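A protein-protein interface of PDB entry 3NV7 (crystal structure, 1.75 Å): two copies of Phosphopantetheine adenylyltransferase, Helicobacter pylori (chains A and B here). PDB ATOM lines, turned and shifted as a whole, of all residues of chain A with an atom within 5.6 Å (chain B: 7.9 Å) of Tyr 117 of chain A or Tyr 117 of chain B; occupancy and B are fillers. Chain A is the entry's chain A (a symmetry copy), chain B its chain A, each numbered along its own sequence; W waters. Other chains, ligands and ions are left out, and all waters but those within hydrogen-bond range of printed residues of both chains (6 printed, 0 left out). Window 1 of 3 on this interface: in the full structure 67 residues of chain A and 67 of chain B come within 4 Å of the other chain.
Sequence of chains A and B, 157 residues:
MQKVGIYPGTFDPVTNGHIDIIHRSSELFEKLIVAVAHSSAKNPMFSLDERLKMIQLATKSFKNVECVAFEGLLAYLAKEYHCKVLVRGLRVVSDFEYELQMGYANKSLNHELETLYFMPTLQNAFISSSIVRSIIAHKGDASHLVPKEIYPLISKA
Printed residues of chain B that touch a printed residue of chain A: Arg 24, Leu 86, Val 87, Arg 88, Gly 89, Leu 90, Val 92, Ser 94, Asp 95, Tyr 98, Glu 114, Thr 115, Leu 116, Tyr 117, Phe 118, Met 119 and Pro 120.
Hydrophobic or aromatic side chains of chain A within 4 Å of the printed part of chain B: Leu 90, Tyr 98, Leu 116, Tyr 117, Phe 118 and Met 119.
Among the printed residues, Asp or Glu carboxylates within 4 Å of a Lys or Arg side-chain nitrogen of the other chain: Arg 88 of chain A with Asp 95 of chain B (2.3 Å) and Asp 95 of chain A with Arg 88 of chain B (2.3 Å).
Arg 88 of chain A touches Tyr 117 of chain B (O to CA, 3.3 Å).
Phe 118 of chain B touches Leu 116 of chain A (CZ to CD2, 3.5 Å).
Tyr 117 of chain A touches Leu 90 of chain B.
CD1 of Leu 90 of chain B touches SD of Met 119 of chain A, 3.8 Å away.
OD2 of Asp 95 of chain B lies within hydrogen-bond range of OH of Tyr 117 of chain B (2.7 Å).
OE2 of Glu 99 of chain A sits at hydrogen-bond distance from OH of Tyr 117 of chain A (2.7 Å).
Water W1 lies within hydrogen-bond range of the side-chain carboxylate (OD1) of Asp 95 of chain A (2.6 Å), the backbone NH (N) of Tyr 98 of chain A (3.0 Å) and the guanidinium group (NH2) of Arg 88 of chain B (3.4 Å).
O of Leu 116 of chain A lies within hydrogen-bond range of N of Arg 88 of chain B (2.9 Å).
The backbone NH (N) of Leu 116 of chain A lies within hydrogen-bond range of the backbone carbonyl oxygen (O) of Leu 86 of chain B, at 2.8 Å.
The side-chain sulfur of Met 119 of chain B is in hydrogen-bond range of the backbone NH of Ser 94 of chain A (3.8 Å).
N of Leu 90 of chain A is in hydrogen-bond range of O of Phe 118 of chain B.
The guanidinium group of Arg 24 of chain B is in hydrogen-bond range of the backbone carbonyl oxygen of Met 119 of chain A.
The backbone NH (N) of Phe 118 of chain B is in hydrogen-bond range of the backbone carbonyl oxygen (O) of Arg 88 of chain A, at 3.0 Å.
SD of Met 119 of chain A sits close to O of Val 92 of chain B, 3.2 Å away.
O of Phe 118 of chain A sits at hydrogen-bond distance from N of Leu 90 of chain B, 2.9 Å away.
O of Arg 88 of chain B lies within hydrogen-bond range of N of Phe 118 of chain A (3.0 Å).
O of Leu 116 of chain B is in hydrogen-bond range of N of Arg 88 of chain A, 2.9 Å away.
The backbone NH of Ser 94 of chain B lies within hydrogen-bond range of the side-chain sulfur of Met 119 of chain A (3.8 Å).
Arg 88 of chain A touches Asp 95 of chain B, and with the chains exchanged Asp 95 of chain A touches Arg 88 of chain B.
Arg 88 of chain A touches Tyr 117 of chain B, and with the chains exchanged Tyr 117 of chain A touches Arg 88 of chain B.
Printed residues of chain B within 4 Å of Leu 116 of chain A: Leu 86 (2.8 Å), Val 87 (3.5 Å), Arg 88 (2.9 Å), Tyr 117 (3.8 Å) and Phe 118 (3.5 Å).
Met 102 of chain B touches none of the printed residues of chain A.
The nearest residue of chain B that does not touch Tyr 117 of chain A is Thr 115 of chain B (4.2 Å).
The nearest residue of chain A that does not touch Tyr 117 of chain B is Thr 115 of chain A (4.2 Å).
The nearest printed residue of chain A that does not touch Leu 86 of chain B is Tyr 117 of chain A (5.6 Å).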
ATOM      1  N   ARG A  88      -9.950  -9.782 -28.870  1.00  0.00           N
ATOM      2  CA  ARG A  88      -9.425  -8.414 -28.694  1.00  0.00           C
ATOM      3  C   ARG A  88      -8.843  -8.231 -27.282  1.00  0.00           C
ATOM      4  O   ARG A  88      -9.350  -8.819 -26.343  1.00  0.00           O
ATOM      5  CB  ARG A  88     -10.542  -7.409 -28.936  1.00  0.00           C
ATOM      6  CG  ARG A  88     -10.040  -5.963 -29.112  1.00  0.00           C
ATOM      7  CD  ARG A  88     -10.960  -5.308 -30.119  1.00  0.00           C
ATOM      8  NE  ARG A  88     -10.806  -3.870 -30.145  1.00  0.00           N
ATOM      9  CZ  ARG A  88     -10.056  -3.209 -31.017  1.00  0.00           C
ATOM     10  NH1 ARG A  88      -9.353  -3.857 -31.928  1.00  0.00           N
ATOM     11  NH2 ARG A  88      -9.998  -1.898 -30.955  1.00  0.00           N
ATOM     12  N   GLY A  89      -7.784  -7.434 -27.140  1.00  0.00           N
ATOM     13  CA  GLY A  89      -7.268  -7.103 -25.818  1.00  0.00           C
ATOM     14  C   GLY A  89      -7.959  -5.842 -25.318  1.00  0.00           C
ATOM     15  O   GLY A  89      -8.205  -4.917 -26.091  1.00  0.00           O
ATOM     16  N   LEU A  90      -8.297  -5.800 -24.037  1.00  0.00           N
ATOM     17  CA  LEU A  90      -8.866  -4.598 -23.431  1.00  0.00           C
ATOM     18  C   LEU A  90      -7.752  -3.605 -23.188  1.00  0.00           C
ATOM     19  O   LEU A  90      -6.635  -4.014 -22.880  1.00  0.00           O
ATOM     20  CB  LEU A  90      -9.513  -4.954 -22.096  1.00  0.00           C
ATOM     21  CG  LEU A  90     -10.815  -5.724 -22.212  1.00  0.00           C
ATOM     22  CD1 LEU A  90     -11.133  -6.322 -20.838  1.00  0.00           C
ATOM     23  CD2 LEU A  90     -11.941  -4.752 -22.644  1.00  0.00           C
ATOM     24  N   SER A  94     -10.086  -3.259 -15.206  1.00  0.00           N
ATOM     25  CA  SER A  94     -11.228  -3.151 -14.324  1.00  0.00           C
ATOM     26  C   SER A  94     -11.338  -4.454 -13.569  1.00  0.00           C
ATOM     27  O   SER A  94     -10.452  -5.304 -13.685  1.00  0.00           O
ATOM     28  CB  SER A  94     -12.500  -2.848 -15.119  1.00  0.00           C
ATOM     29  OG  SER A  94     -12.718  -3.780 -16.155  1.00  0.00           O
ATOM     30  N   ASP A  95     -12.398  -4.604 -12.775  1.00  0.00           N
ATOM     31  CA  ASP A  95     -12.729  -5.876 -12.135  1.00  0.00           C
ATOM     32  C   ASP A  95     -11.652  -6.300 -11.147  1.00  0.00           C
ATOM     33  O   ASP A  95     -11.259  -7.471 -11.078  1.00  0.00           O
ATOM     34  CB  ASP A  95     -12.941  -6.963 -13.199  1.00  0.00           C
ATOM     35  CG  ASP A  95     -13.985  -7.973 -12.803  1.00  0.00           C
ATOM     36  OD1 ASP A  95     -14.766  -7.723 -11.844  1.00  0.00           O
ATOM     37  OD2 ASP A  95     -14.022  -9.040 -13.446  1.00  0.00           O
ATOM     38  N   TYR A  98     -12.221  -9.171  -8.343  1.00  0.00           N
ATOM     39  CA  TYR A  98     -12.233 -10.454  -9.034  1.00  0.00           C
ATOM     40  C   TYR A  98     -10.816 -10.878  -9.472  1.00  0.00           C
ATOM     41  O   TYR A  98     -10.406 -12.009  -9.267  1.00  0.00           O
ATOM     42  CB  TYR A  98     -13.146 -10.364 -10.254  1.00  0.00           C
ATOM     43  CG  TYR A  98     -13.130 -11.582 -11.130  1.00  0.00           C
ATOM     44  CD1 TYR A  98     -12.284 -11.654 -12.243  1.00  0.00           C
ATOM     45  CD2 TYR A  98     -13.948 -12.675 -10.848  1.00  0.00           C
ATOM     46  CE1 TYR A  98     -12.267 -12.772 -13.037  1.00  0.00           C
ATOM     47  CE2 TYR A  98     -13.944 -13.798 -11.653  1.00  0.00           C
ATOM     48  CZ  TYR A  98     -13.092 -13.838 -12.739  1.00  0.00           C
ATOM     49  OH  TYR A  98     -13.070 -14.937 -13.555  1.00  0.00           O
ATOM     50  N   GLU A  99     -10.074  -9.951 -10.063  1.00  0.00           N
ATOM     51  CA  GLU A  99      -8.741 -10.264 -10.567  1.00  0.00           C
ATOM     52  C   GLU A  99      -7.778 -10.543  -9.422  1.00  0.00           C
ATOM     53  O   GLU A  99      -6.881 -11.377  -9.556  1.00  0.00           O
ATOM     54  CB  GLU A  99      -8.231  -9.170 -11.501  1.00  0.00           C
ATOM     55  CG  GLU A  99      -8.970  -9.107 -12.868  1.00  0.00           C
ATOM     56  CD  GLU A  99      -8.789 -10.368 -13.755  1.00  0.00           C
ATOM     57  OE1 GLU A  99      -7.971 -11.280 -13.439  1.00  0.00           O
ATOM     58  OE2 GLU A  99      -9.482 -10.445 -14.783  1.00  0.00           O
ATOM     59  N   THR A 115      -9.862 -15.959 -17.821  1.00  0.00           N
ATOM     60  CA  THR A 115     -11.193 -15.336 -17.857  1.00  0.00           C
ATOM     61  C   THR A 115     -11.457 -14.694 -19.222  1.00  0.00           C
ATOM     62  O   THR A 115     -10.640 -13.883 -19.712  1.00  0.00           O
ATOM     63  CB  THR A 115     -11.341 -14.274 -16.744  1.00  0.00           C
ATOM     64  OG1 THR A 115     -11.147 -14.896 -15.492  1.00  0.00           O
ATOM     65  CG2 THR A 115     -12.736 -13.644 -16.763  1.00  0.00           C
ATOM     66  N   LEU A 116     -12.582 -15.042 -19.841  1.00  0.00           N
ATOM     67  CA  LEU A 116     -13.010 -14.390 -21.079  1.00  0.00           C
ATOM     68  C   LEU A 116     -14.033 -13.328 -20.731  1.00  0.00           C
ATOM     69  O   LEU A 116     -15.034 -13.639 -20.040  1.00  0.00           O
ATOM     70  CB  LEU A 116     -13.670 -15.408 -22.010  1.00  0.00           C
ATOM     71  CG  LEU A 116     -12.812 -16.601 -22.432  1.00  0.00           C
ATOM     72  CD1 LEU A 116     -13.651 -17.507 -23.353  1.00  0.00           C
ATOM     73  CD2 LEU A 116     -11.497 -16.154 -23.091  1.00  0.00           C
ATOM     74  N   TYR A 117     -13.797 -12.097 -21.211  1.00  0.00           N
ATOM     75  CA  TYR A 117     -14.718 -10.990 -20.976  1.00  0.00           C
ATOM     76  C   TYR A 117     -15.622 -10.697 -22.150  1.00  0.00           C
ATOM     77  O   TYR A 117     -15.189 -10.700 -23.326  1.00  0.00           O
ATOM     78  CB  TYR A 117     -13.963  -9.724 -20.572  1.00  0.00           C
ATOM     79  CG  TYR A 117     -13.466  -9.744 -19.140  1.00  0.00           C
ATOM     80  CD1 TYR A 117     -14.291  -9.340 -18.082  1.00  0.00           C
ATOM     81  CD2 TYR A 117     -12.159 -10.174 -18.839  1.00  0.00           C
ATOM     82  CE1 TYR A 117     -13.820  -9.352 -16.754  1.00  0.00           C
ATOM     83  CE2 TYR A 117     -11.685 -10.190 -17.530  1.00  0.00           C
ATOM     84  CZ  TYR A 117     -12.520  -9.768 -16.486  1.00  0.00           C
ATOM     85  OH  TYR A 117     -12.035  -9.788 -15.186  1.00  0.00           O
ATOM     86  N   PHE A 118     -16.880 -10.438 -21.809  1.00  0.00           N
ATOM     87  CA  PHE A 118     -17.930 -10.120 -22.789  1.00  0.00           C
ATOM     88  C   PHE A 118     -18.400  -8.713 -22.550  1.00  0.00           C
ATOM     89  O   PHE A 118     -18.842  -8.362 -21.443  1.00  0.00           O
ATOM     90  CB  PHE A 118     -19.087 -11.118 -22.657  1.00  0.00           C
ATOM     91  CG  PHE A 118     -18.725 -12.513 -23.112  1.00  0.00           C
ATOM     92  CD1 PHE A 118     -19.108 -12.972 -24.373  1.00  0.00           C
ATOM     93  CD2 PHE A 118     -17.976 -13.364 -22.283  1.00  0.00           C
ATOM     94  CE1 PHE A 118     -18.783 -14.288 -24.798  1.00  0.00           C
ATOM     95  CE2 PHE A 118     -17.639 -14.645 -22.681  1.00  0.00           C
ATOM     96  CZ  PHE A 118     -18.055 -15.119 -23.936  1.00  0.00           C
ATOM     97  N   MET A 119     -18.314  -7.904 -23.602  1.00  0.00           N
ATOM     98  CA  MET A 119     -18.775  -6.525 -23.542  1.00  0.00           C
ATOM     99  C   MET A 119     -20.291  -6.498 -23.650  1.00  0.00           C
ATOM    100  O   MET A 119     -20.863  -7.129 -24.560  1.00  0.00           O
ATOM    101  CB  MET A 119     -18.176  -5.749 -24.709  1.00  0.00           C
ATOM    102  CG  MET A 119     -18.526  -4.293 -24.711  1.00  0.00           C
ATOM    103  SD  MET A 119     -17.377  -3.451 -23.648  1.00  0.00           S
ATOM    104  CE  MET A 119     -16.066  -3.454 -24.837  1.00  0.00           C
ATOM    105  N   ILE B  21     -25.127 -12.820 -21.731  1.00  0.00           N
ATOM    106  CA  ILE B  21     -23.806 -13.446 -21.553  1.00  0.00           C
ATOM    107  C   ILE B  21     -23.878 -14.985 -21.593  1.00  0.00           C
ATOM    108  O   ILE B  21     -23.014 -15.622 -22.189  1.00  0.00           O
ATOM    109  CB  ILE B  21     -23.128 -12.991 -20.259  1.00  0.00           C
ATOM    110  CG1 ILE B  21     -22.861 -11.480 -20.315  1.00  0.00           C
ATOM    111  CG2 ILE B  21     -21.838 -13.789 -19.988  1.00  0.00           C
ATOM    112  CD1 ILE B  21     -22.681 -10.837 -18.956  1.00  0.00           C
ATOM    113  N   ARG B  24     -24.424 -15.982 -25.249  1.00  0.00           N
ATOM    114  CA  ARG B  24     -23.225 -15.812 -26.067  1.00  0.00           C
ATOM    115  C   ARG B  24     -22.131 -16.789 -25.669  1.00  0.00           C
ATOM    116  O   ARG B  24     -21.490 -17.375 -26.535  1.00  0.00           O
ATOM    117  CB  ARG B  24     -22.709 -14.359 -25.989  1.00  0.00           C
ATOM    118  CG  ARG B  24     -23.674 -13.362 -26.630  1.00  0.00           C
ATOM    119  CD  ARG B  24     -23.504 -11.941 -26.103  1.00  0.00           C
ATOM    120  NE  ARG B  24     -22.169 -11.399 -26.315  1.00  0.00           N
ATOM    121  CZ  ARG B  24     -21.738 -10.248 -25.796  1.00  0.00           C
ATOM    122  NH1 ARG B  24     -20.499  -9.849 -26.052  1.00  0.00           N
ATOM    123  NH2 ARG B  24     -22.545  -9.485 -25.038  1.00  0.00           N
ATOM    124  N   LEU B  86     -13.096 -19.310 -17.365  1.00  0.00           N
ATOM    125  CA  LEU B  86     -14.241 -18.660 -16.759  1.00  0.00           C
ATOM    126  C   LEU B  86     -14.763 -17.582 -17.682  1.00  0.00           C
ATOM    127  O   LEU B  86     -14.026 -17.068 -18.542  1.00  0.00           O
ATOM    128  CB  LEU B  86     -13.880 -18.057 -15.394  1.00  0.00           C
ATOM    129  CG  LEU B  86     -13.210 -19.003 -14.396  1.00  0.00           C
ATOM    130  CD1 LEU B  86     -13.003 -18.245 -13.085  1.00  0.00           C
ATOM    131  CD2 LEU B  86     -14.025 -20.266 -14.178  1.00  0.00           C
ATOM    132  N   VAL B  87     -16.021 -17.206 -17.471  1.00  0.00           N
ATOM    133  CA  VAL B  87     -16.701 -16.229 -18.307  1.00  0.00           C
ATOM    134  C   VAL B  87     -17.102 -15.068 -17.401  1.00  0.00           C
ATOM    135  O   VAL B  87     -17.581 -15.283 -16.280  1.00  0.00           O
ATOM    136  CB  VAL B  87     -17.944 -16.933 -18.937  1.00  0.00           C
ATOM    137  CG1 VAL B  87     -19.021 -15.952 -19.401  1.00  0.00           C
ATOM    138  CG2 VAL B  87     -17.493 -17.882 -20.081  1.00  0.00           C
ATOM    139  N   ARG B  88     -16.930 -13.832 -17.858  1.00  0.00           N
ATOM    140  CA  ARG B  88     -17.384 -12.676 -17.060  1.00  0.00           C
ATOM    141  C   ARG B  88     -17.930 -11.565 -17.973  1.00  0.00           C
ATOM    142  O   ARG B  88     -17.435 -11.395 -19.073  1.00  0.00           O
ATOM    143  CB  ARG B  88     -16.224 -12.150 -16.227  1.00  0.00           C
ATOM    144  CG  ARG B  88     -16.657 -11.174 -15.117  1.00  0.00           C
ATOM    145  CD  ARG B  88     -15.726 -11.410 -13.949  1.00  0.00           C
ATOM    146  NE  ARG B  88     -15.809 -10.357 -12.962  1.00  0.00           N
ATOM    147  CZ  ARG B  88     -16.542 -10.416 -11.857  1.00  0.00           C
ATOM    148  NH1 ARG B  88     -17.294 -11.473 -11.604  1.00  0.00           N
ATOM    149  NH2 ARG B  88     -16.535  -9.401 -11.023  1.00  0.00           N
ATOM    150  N   GLY B  89     -18.946 -10.828 -17.524  1.00  0.00           N
ATOM    151  CA  GLY B  89     -19.419  -9.671 -18.271  1.00  0.00           C
ATOM    152  C   GLY B  89     -18.658  -8.436 -17.808  1.00  0.00           C
ATOM    153  O   GLY B  89     -18.381  -8.283 -16.620  1.00  0.00           O
ATOM    154  N   LEU B  90     -18.294  -7.562 -18.737  1.00  0.00           N
ATOM    155  CA  LEU B  90     -17.655  -6.294 -18.389  1.00  0.00           C
ATOM    156  C   LEU B  90     -18.714  -5.342 -17.882  1.00  0.00           C
ATOM    157  O   LEU B  90     -19.843  -5.383 -18.363  1.00  0.00           O
ATOM    158  CB  LEU B  90     -17.001  -5.694 -19.630  1.00  0.00           C
ATOM    159  CG  LEU B  90     -15.741  -6.405 -20.085  1.00  0.00           C
ATOM    160  CD1 LEU B  90     -15.427  -5.941 -21.512  1.00  0.00           C
ATOM    161  CD2 LEU B  90     -14.577  -6.031 -19.134  1.00  0.00           C
ATOM    162  N   ARG B  91     -18.361  -4.523 -16.894  1.00  0.00           N
ATOM    163  CA  ARG B  91     -19.215  -3.405 -16.464  1.00  0.00           C
ATOM    164  C   ARG B  91     -18.656  -2.096 -17.001  1.00  0.00           C
ATOM    165  O   ARG B  91     -18.920  -1.002 -16.505  1.00  0.00           O
ATOM    166  CB  ARG B  91     -19.314  -3.367 -14.942  1.00  0.00           C
ATOM    167  CG  ARG B  91     -19.974  -4.595 -14.367  1.00  0.00           C
ATOM    168  CD  ARG B  91     -21.433  -4.722 -14.783  1.00  0.00           C
ATOM    169  NE  ARG B  91     -22.171  -3.465 -14.637  1.00  0.00           N
ATOM    170  CZ  ARG B  91     -23.408  -3.265 -15.066  1.00  0.00           C
ATOM    171  NH1 ARG B  91     -24.069  -4.271 -15.647  1.00  0.00           N
ATOM    172  NH2 ARG B  91     -23.986  -2.067 -14.889  1.00  0.00           N
ATOM    173  N   VAL B  92     -17.880  -2.201 -18.050  1.00  0.00           N
ATOM    174  CA  VAL B  92     -17.371  -1.009 -18.702  1.00  0.00           C
ATOM    175  C   VAL B  92     -17.657  -1.132 -20.173  1.00  0.00           C
ATOM    176  O   VAL B  92     -17.628  -2.231 -20.740  1.00  0.00           O
ATOM    177  CB  VAL B  92     -15.867  -0.846 -18.446  1.00  0.00           C
ATOM    178  CG1 VAL B  92     -15.622  -0.636 -16.991  1.00  0.00           C
ATOM    179  CG2 VAL B  92     -15.153  -2.078 -18.870  1.00  0.00           C
ATOM    180  N   SER B  94     -16.214   0.156 -23.610  1.00  0.00           N
ATOM    181  CA  SER B  94     -15.052   0.772 -24.212  1.00  0.00           C
ATOM    182  C   SER B  94     -14.992   0.309 -25.649  1.00  0.00           C
ATOM    183  O   SER B  94     -15.921  -0.354 -26.117  1.00  0.00           O
ATOM    184  CB  SER B  94     -13.782   0.400 -23.444  1.00  0.00           C
ATOM    185  OG  SER B  94     -13.630  -0.996 -23.306  1.00  0.00           O
ATOM    186  N   ASP B  95     -13.926   0.679 -26.358  1.00  0.00           N
ATOM    187  CA  ASP B  95     -13.645   0.151 -27.693  1.00  0.00           C
ATOM    188  C   ASP B  95     -14.724   0.554 -28.689  1.00  0.00           C
ATOM    189  O   ASP B  95     -15.172  -0.248 -29.518  1.00  0.00           O
ATOM    190  CB  ASP B  95     -13.507  -1.378 -27.638  1.00  0.00           C
ATOM    191  CG  ASP B  95     -12.508  -1.910 -28.628  1.00  0.00           C
ATOM    192  OD1 ASP B  95     -11.697  -1.121 -29.186  1.00  0.00           O
ATOM    193  OD2 ASP B  95     -12.535  -3.134 -28.868  1.00  0.00           O
ATOM    194  N   PHE B  96     -15.124   1.811 -28.603  1.00  0.00           N
ATOM    195  CA  PHE B  96     -16.277   2.304 -29.325  1.00  0.00           C
ATOM    196  C   PHE B  96     -16.154   2.265 -30.839  1.00  0.00           C
ATOM    197  O   PHE B  96     -17.104   1.857 -31.492  1.00  0.00           O
ATOM    198  CB  PHE B  96     -16.694   3.701 -28.831  1.00  0.00           C
ATOM    199  CG  PHE B  96     -17.203   3.706 -27.417  1.00  0.00           C
ATOM    200  CD1 PHE B  96     -16.341   3.955 -26.354  1.00  0.00           C
ATOM    201  CD2 PHE B  96     -18.544   3.437 -27.147  1.00  0.00           C
ATOM    202  CE1 PHE B  96     -16.792   3.951 -25.037  1.00  0.00           C
ATOM    203  CE2 PHE B  96     -19.012   3.429 -25.838  1.00  0.00           C
ATOM    204  CZ  PHE B  96     -18.128   3.674 -24.772  1.00  0.00           C
ATOM    205  N   TYR B  98     -14.243   0.283 -32.704  1.00  0.00           N
ATOM    206  CA  TYR B  98     -14.308  -1.130 -33.054  1.00  0.00           C
ATOM    207  C   TYR B  98     -15.752  -1.668 -32.987  1.00  0.00           C
ATOM    208  O   TYR B  98     -16.213  -2.347 -33.889  1.00  0.00           O
ATOM    209  CB  TYR B  98     -13.415  -1.927 -32.106  1.00  0.00           C
ATOM    210  CG  TYR B  98     -13.507  -3.416 -32.274  1.00  0.00           C
ATOM    211  CD1 TYR B  98     -14.377  -4.174 -31.482  1.00  0.00           C
ATOM    212  CD2 TYR B  98     -12.739  -4.075 -33.232  1.00  0.00           C
ATOM    213  CE1 TYR B  98     -14.463  -5.533 -31.643  1.00  0.00           C
ATOM    214  CE2 TYR B  98     -12.813  -5.446 -33.389  1.00  0.00           C
ATOM    215  CZ  TYR B  98     -13.687  -6.162 -32.595  1.00  0.00           C
ATOM    216  OH  TYR B  98     -13.779  -7.522 -32.727  1.00  0.00           O
ATOM    217  N   GLU B  99     -16.459  -1.343 -31.912  1.00  0.00           N
ATOM    218  CA  GLU B  99     -17.814  -1.847 -31.724  1.00  0.00           C
ATOM    219  C   GLU B  99     -18.768  -1.237 -32.741  1.00  0.00           C
ATOM    220  O   GLU B  99     -19.708  -1.900 -33.184  1.00  0.00           O
ATOM    221  CB  GLU B  99     -18.288  -1.639 -30.287  1.00  0.00           C
ATOM    222  CG  GLU B  99     -17.573  -2.546 -29.246  1.00  0.00           C
ATOM    223  CD  GLU B  99     -17.832  -4.065 -29.431  1.00  0.00           C
ATOM    224  OE1 GLU B  99     -18.688  -4.488 -30.263  1.00  0.00           O
ATOM    225  OE2 GLU B  99     -17.164  -4.846 -28.734  1.00  0.00           O
ATOM    226  N   MET B 102     -18.178  -3.247 -35.870  1.00  0.00           N
ATOM    227  CA  MET B 102     -18.746  -4.586 -35.715  1.00  0.00           C
ATOM    228  C   MET B 102     -20.251  -4.594 -35.933  1.00  0.00           C
ATOM    229  O   MET B 102     -20.773  -5.516 -36.552  1.00  0.00           O
ATOM    230  CB  MET B 102     -18.382  -5.198 -34.361  1.00  0.00           C
ATOM    231  CG  MET B 102     -16.949  -5.681 -34.288  1.00  0.00           C
ATOM    232  SD  MET B 102     -16.548  -6.860 -35.601  1.00  0.00           S
ATOM    233  CE  MET B 102     -15.556  -5.858 -36.723  1.00  0.00           C
ATOM    234  N   GLU B 114     -18.958 -12.622 -32.794  1.00  0.00           N
ATOM    235  CA  GLU B 114     -18.719 -12.376 -31.382  1.00  0.00           C
ATOM    236  C   GLU B 114     -17.309 -11.848 -31.187  1.00  0.00           C
ATOM    237  O   GLU B 114     -16.414 -12.214 -31.947  1.00  0.00           O
ATOM    238  CB  GLU B 114     -18.851 -13.698 -30.607  1.00  0.00           C
ATOM    239  CG  GLU B 114     -18.526 -13.578 -29.126  1.00  0.00           C
ATOM    240  CD  GLU B 114     -19.538 -12.688 -28.389  1.00  0.00           C
ATOM    241  OE1 GLU B 114     -20.654 -13.176 -28.111  1.00  0.00           O
ATOM    242  OE2 GLU B 114     -19.248 -11.506 -28.115  1.00  0.00           O
ATOM    243  N   THR B 115     -17.113 -10.983 -30.190  1.00  0.00           N
ATOM    244  CA  THR B 115     -15.753 -10.612 -29.770  1.00  0.00           C
ATOM    245  C   THR B 115     -15.484 -11.065 -28.333  1.00  0.00           C
ATOM    246  O   THR B 115     -16.270 -10.755 -27.410  1.00  0.00           O
ATOM    247  CB  THR B 115     -15.533  -9.086 -29.886  1.00  0.00           C
ATOM    248  OG1 THR B 115     -15.733  -8.696 -31.227  1.00  0.00           O
ATOM    249  CG2 THR B 115     -14.109  -8.702 -29.476  1.00  0.00           C
ATOM    250  N   LEU B 116     -14.390 -11.794 -28.129  1.00  0.00           N
ATOM    251  CA  LEU B 116     -13.954 -12.164 -26.782  1.00  0.00           C
ATOM    252  C   LEU B 116     -12.874 -11.194 -26.347  1.00  0.00           C
ATOM    253  O   LEU B 116     -11.876 -11.010 -27.087  1.00  0.00           O
ATOM    254  CB  LEU B 116     -13.362 -13.574 -26.788  1.00  0.00           C
ATOM    255  CG  LEU B 116     -14.286 -14.697 -27.259  1.00  0.00           C
ATOM    256  CD1 LEU B 116     -13.510 -16.027 -27.201  1.00  0.00           C
ATOM    257  CD2 LEU B 116     -15.590 -14.744 -26.446  1.00  0.00           C
ATOM    258  N   TYR B 117     -13.058 -10.595 -25.161  1.00  0.00           N
ATOM    259  CA  TYR B 117     -12.079  -9.663 -24.609  1.00  0.00           C
ATOM    260  C   TYR B 117     -11.184 -10.279 -23.560  1.00  0.00           C
ATOM    261  O   TYR B 117     -11.639 -11.049 -22.682  1.00  0.00           O
ATOM    262  CB  TYR B 117     -12.763  -8.419 -24.045  1.00  0.00           C
ATOM    263  CG  TYR B 117     -13.233  -7.448 -25.110  1.00  0.00           C
ATOM    264  CD1 TYR B 117     -12.369  -6.479 -25.639  1.00  0.00           C
ATOM    265  CD2 TYR B 117     -14.554  -7.499 -25.597  1.00  0.00           C
ATOM    266  CE1 TYR B 117     -12.815  -5.575 -26.622  1.00  0.00           C
ATOM    267  CE2 TYR B 117     -15.003  -6.610 -26.569  1.00  0.00           C
ATOM    268  CZ  TYR B 117     -14.129  -5.638 -27.075  1.00  0.00           C
ATOM    269  OH  TYR B 117     -14.589  -4.757 -28.043  1.00  0.00           O
ATOM    270  N   PHE B 118      -9.908  -9.920 -23.663  1.00  0.00           N
ATOM    271  CA  PHE B 118      -8.863 -10.394 -22.743  1.00  0.00           C
ATOM    272  C   PHE B 118      -8.320  -9.216 -21.985  1.00  0.00           C
ATOM    273  O   PHE B 118      -7.841  -8.235 -22.578  1.00  0.00           O
ATOM    274  CB  PHE B 118      -7.755 -11.101 -23.532  1.00  0.00           C
ATOM    275  CG  PHE B 118      -8.193 -12.420 -24.124  1.00  0.00           C
ATOM    276  CD1 PHE B 118      -7.858 -13.625 -23.505  1.00  0.00           C
ATOM    277  CD2 PHE B 118      -8.967 -12.457 -25.295  1.00  0.00           C
ATOM    278  CE1 PHE B 118      -8.255 -14.868 -24.068  1.00  0.00           C
ATOM    279  CE2 PHE B 118      -9.374 -13.655 -25.853  1.00  0.00           C
ATOM    280  CZ  PHE B 118      -9.006 -14.869 -25.250  1.00  0.00           C
ATOM    281  N   MET B 119      -8.386  -9.319 -20.660  1.00  0.00           N
ATOM    282  CA  MET B 119      -7.856  -8.281 -19.788  1.00  0.00           C
ATOM    283  C   MET B 119      -6.343  -8.409 -19.719  1.00  0.00           C
ATOM    284  O   MET B 119      -5.821  -9.514 -19.478  1.00  0.00           O
ATOM    285  CB  MET B 119      -8.439  -8.461 -18.392  1.00  0.00           C
ATOM    286  CG  MET B 119      -8.018  -7.403 -17.420  1.00  0.00           C
ATOM    287  SD  MET B 119      -9.103  -6.010 -17.620  1.00  0.00           S
ATOM    288  CE  MET B 119     -10.436  -6.746 -16.716  1.00  0.00           C
ATOM    289  N   PRO B 120      -5.630  -7.293 -19.928  1.00  0.00           N
ATOM    290  CA  PRO B 120      -4.159  -7.359 -19.908  1.00  0.00           C
ATOM    291  C   PRO B 120      -3.629  -7.612 -18.528  1.00  0.00           C
ATOM    292  O   PRO B 120      -4.268  -7.202 -17.545  1.00  0.00           O
ATOM    293  CB  PRO B 120      -3.739  -5.959 -20.342  1.00  0.00           C
ATOM    294  CG  PRO B 120      -4.863  -5.063 -19.910  1.00  0.00           C
ATOM    295  CD  PRO B 120      -6.098  -5.924 -20.223  1.00  0.00           C
HETATM  296  O   HOH W   1     -14.420  -7.419  -9.300  1.00  0.00           O
HETATM  297  O   HOH W   2     -11.979   0.828 -30.861  1.00  0.00           O
HETATM  298  O   HOH W   3     -15.900 -15.120 -13.793  1.00  0.00           O
HETATM  299  O   HOH W   4      -9.044 -11.765 -19.282  1.00  0.00           O
HETATM  300  O   HOH W   5     -17.751  -8.820 -26.277  1.00  0.00           O
HETATM  301  O   HOH W   6     -15.741  -4.570 -15.650  1.00  0.00           O
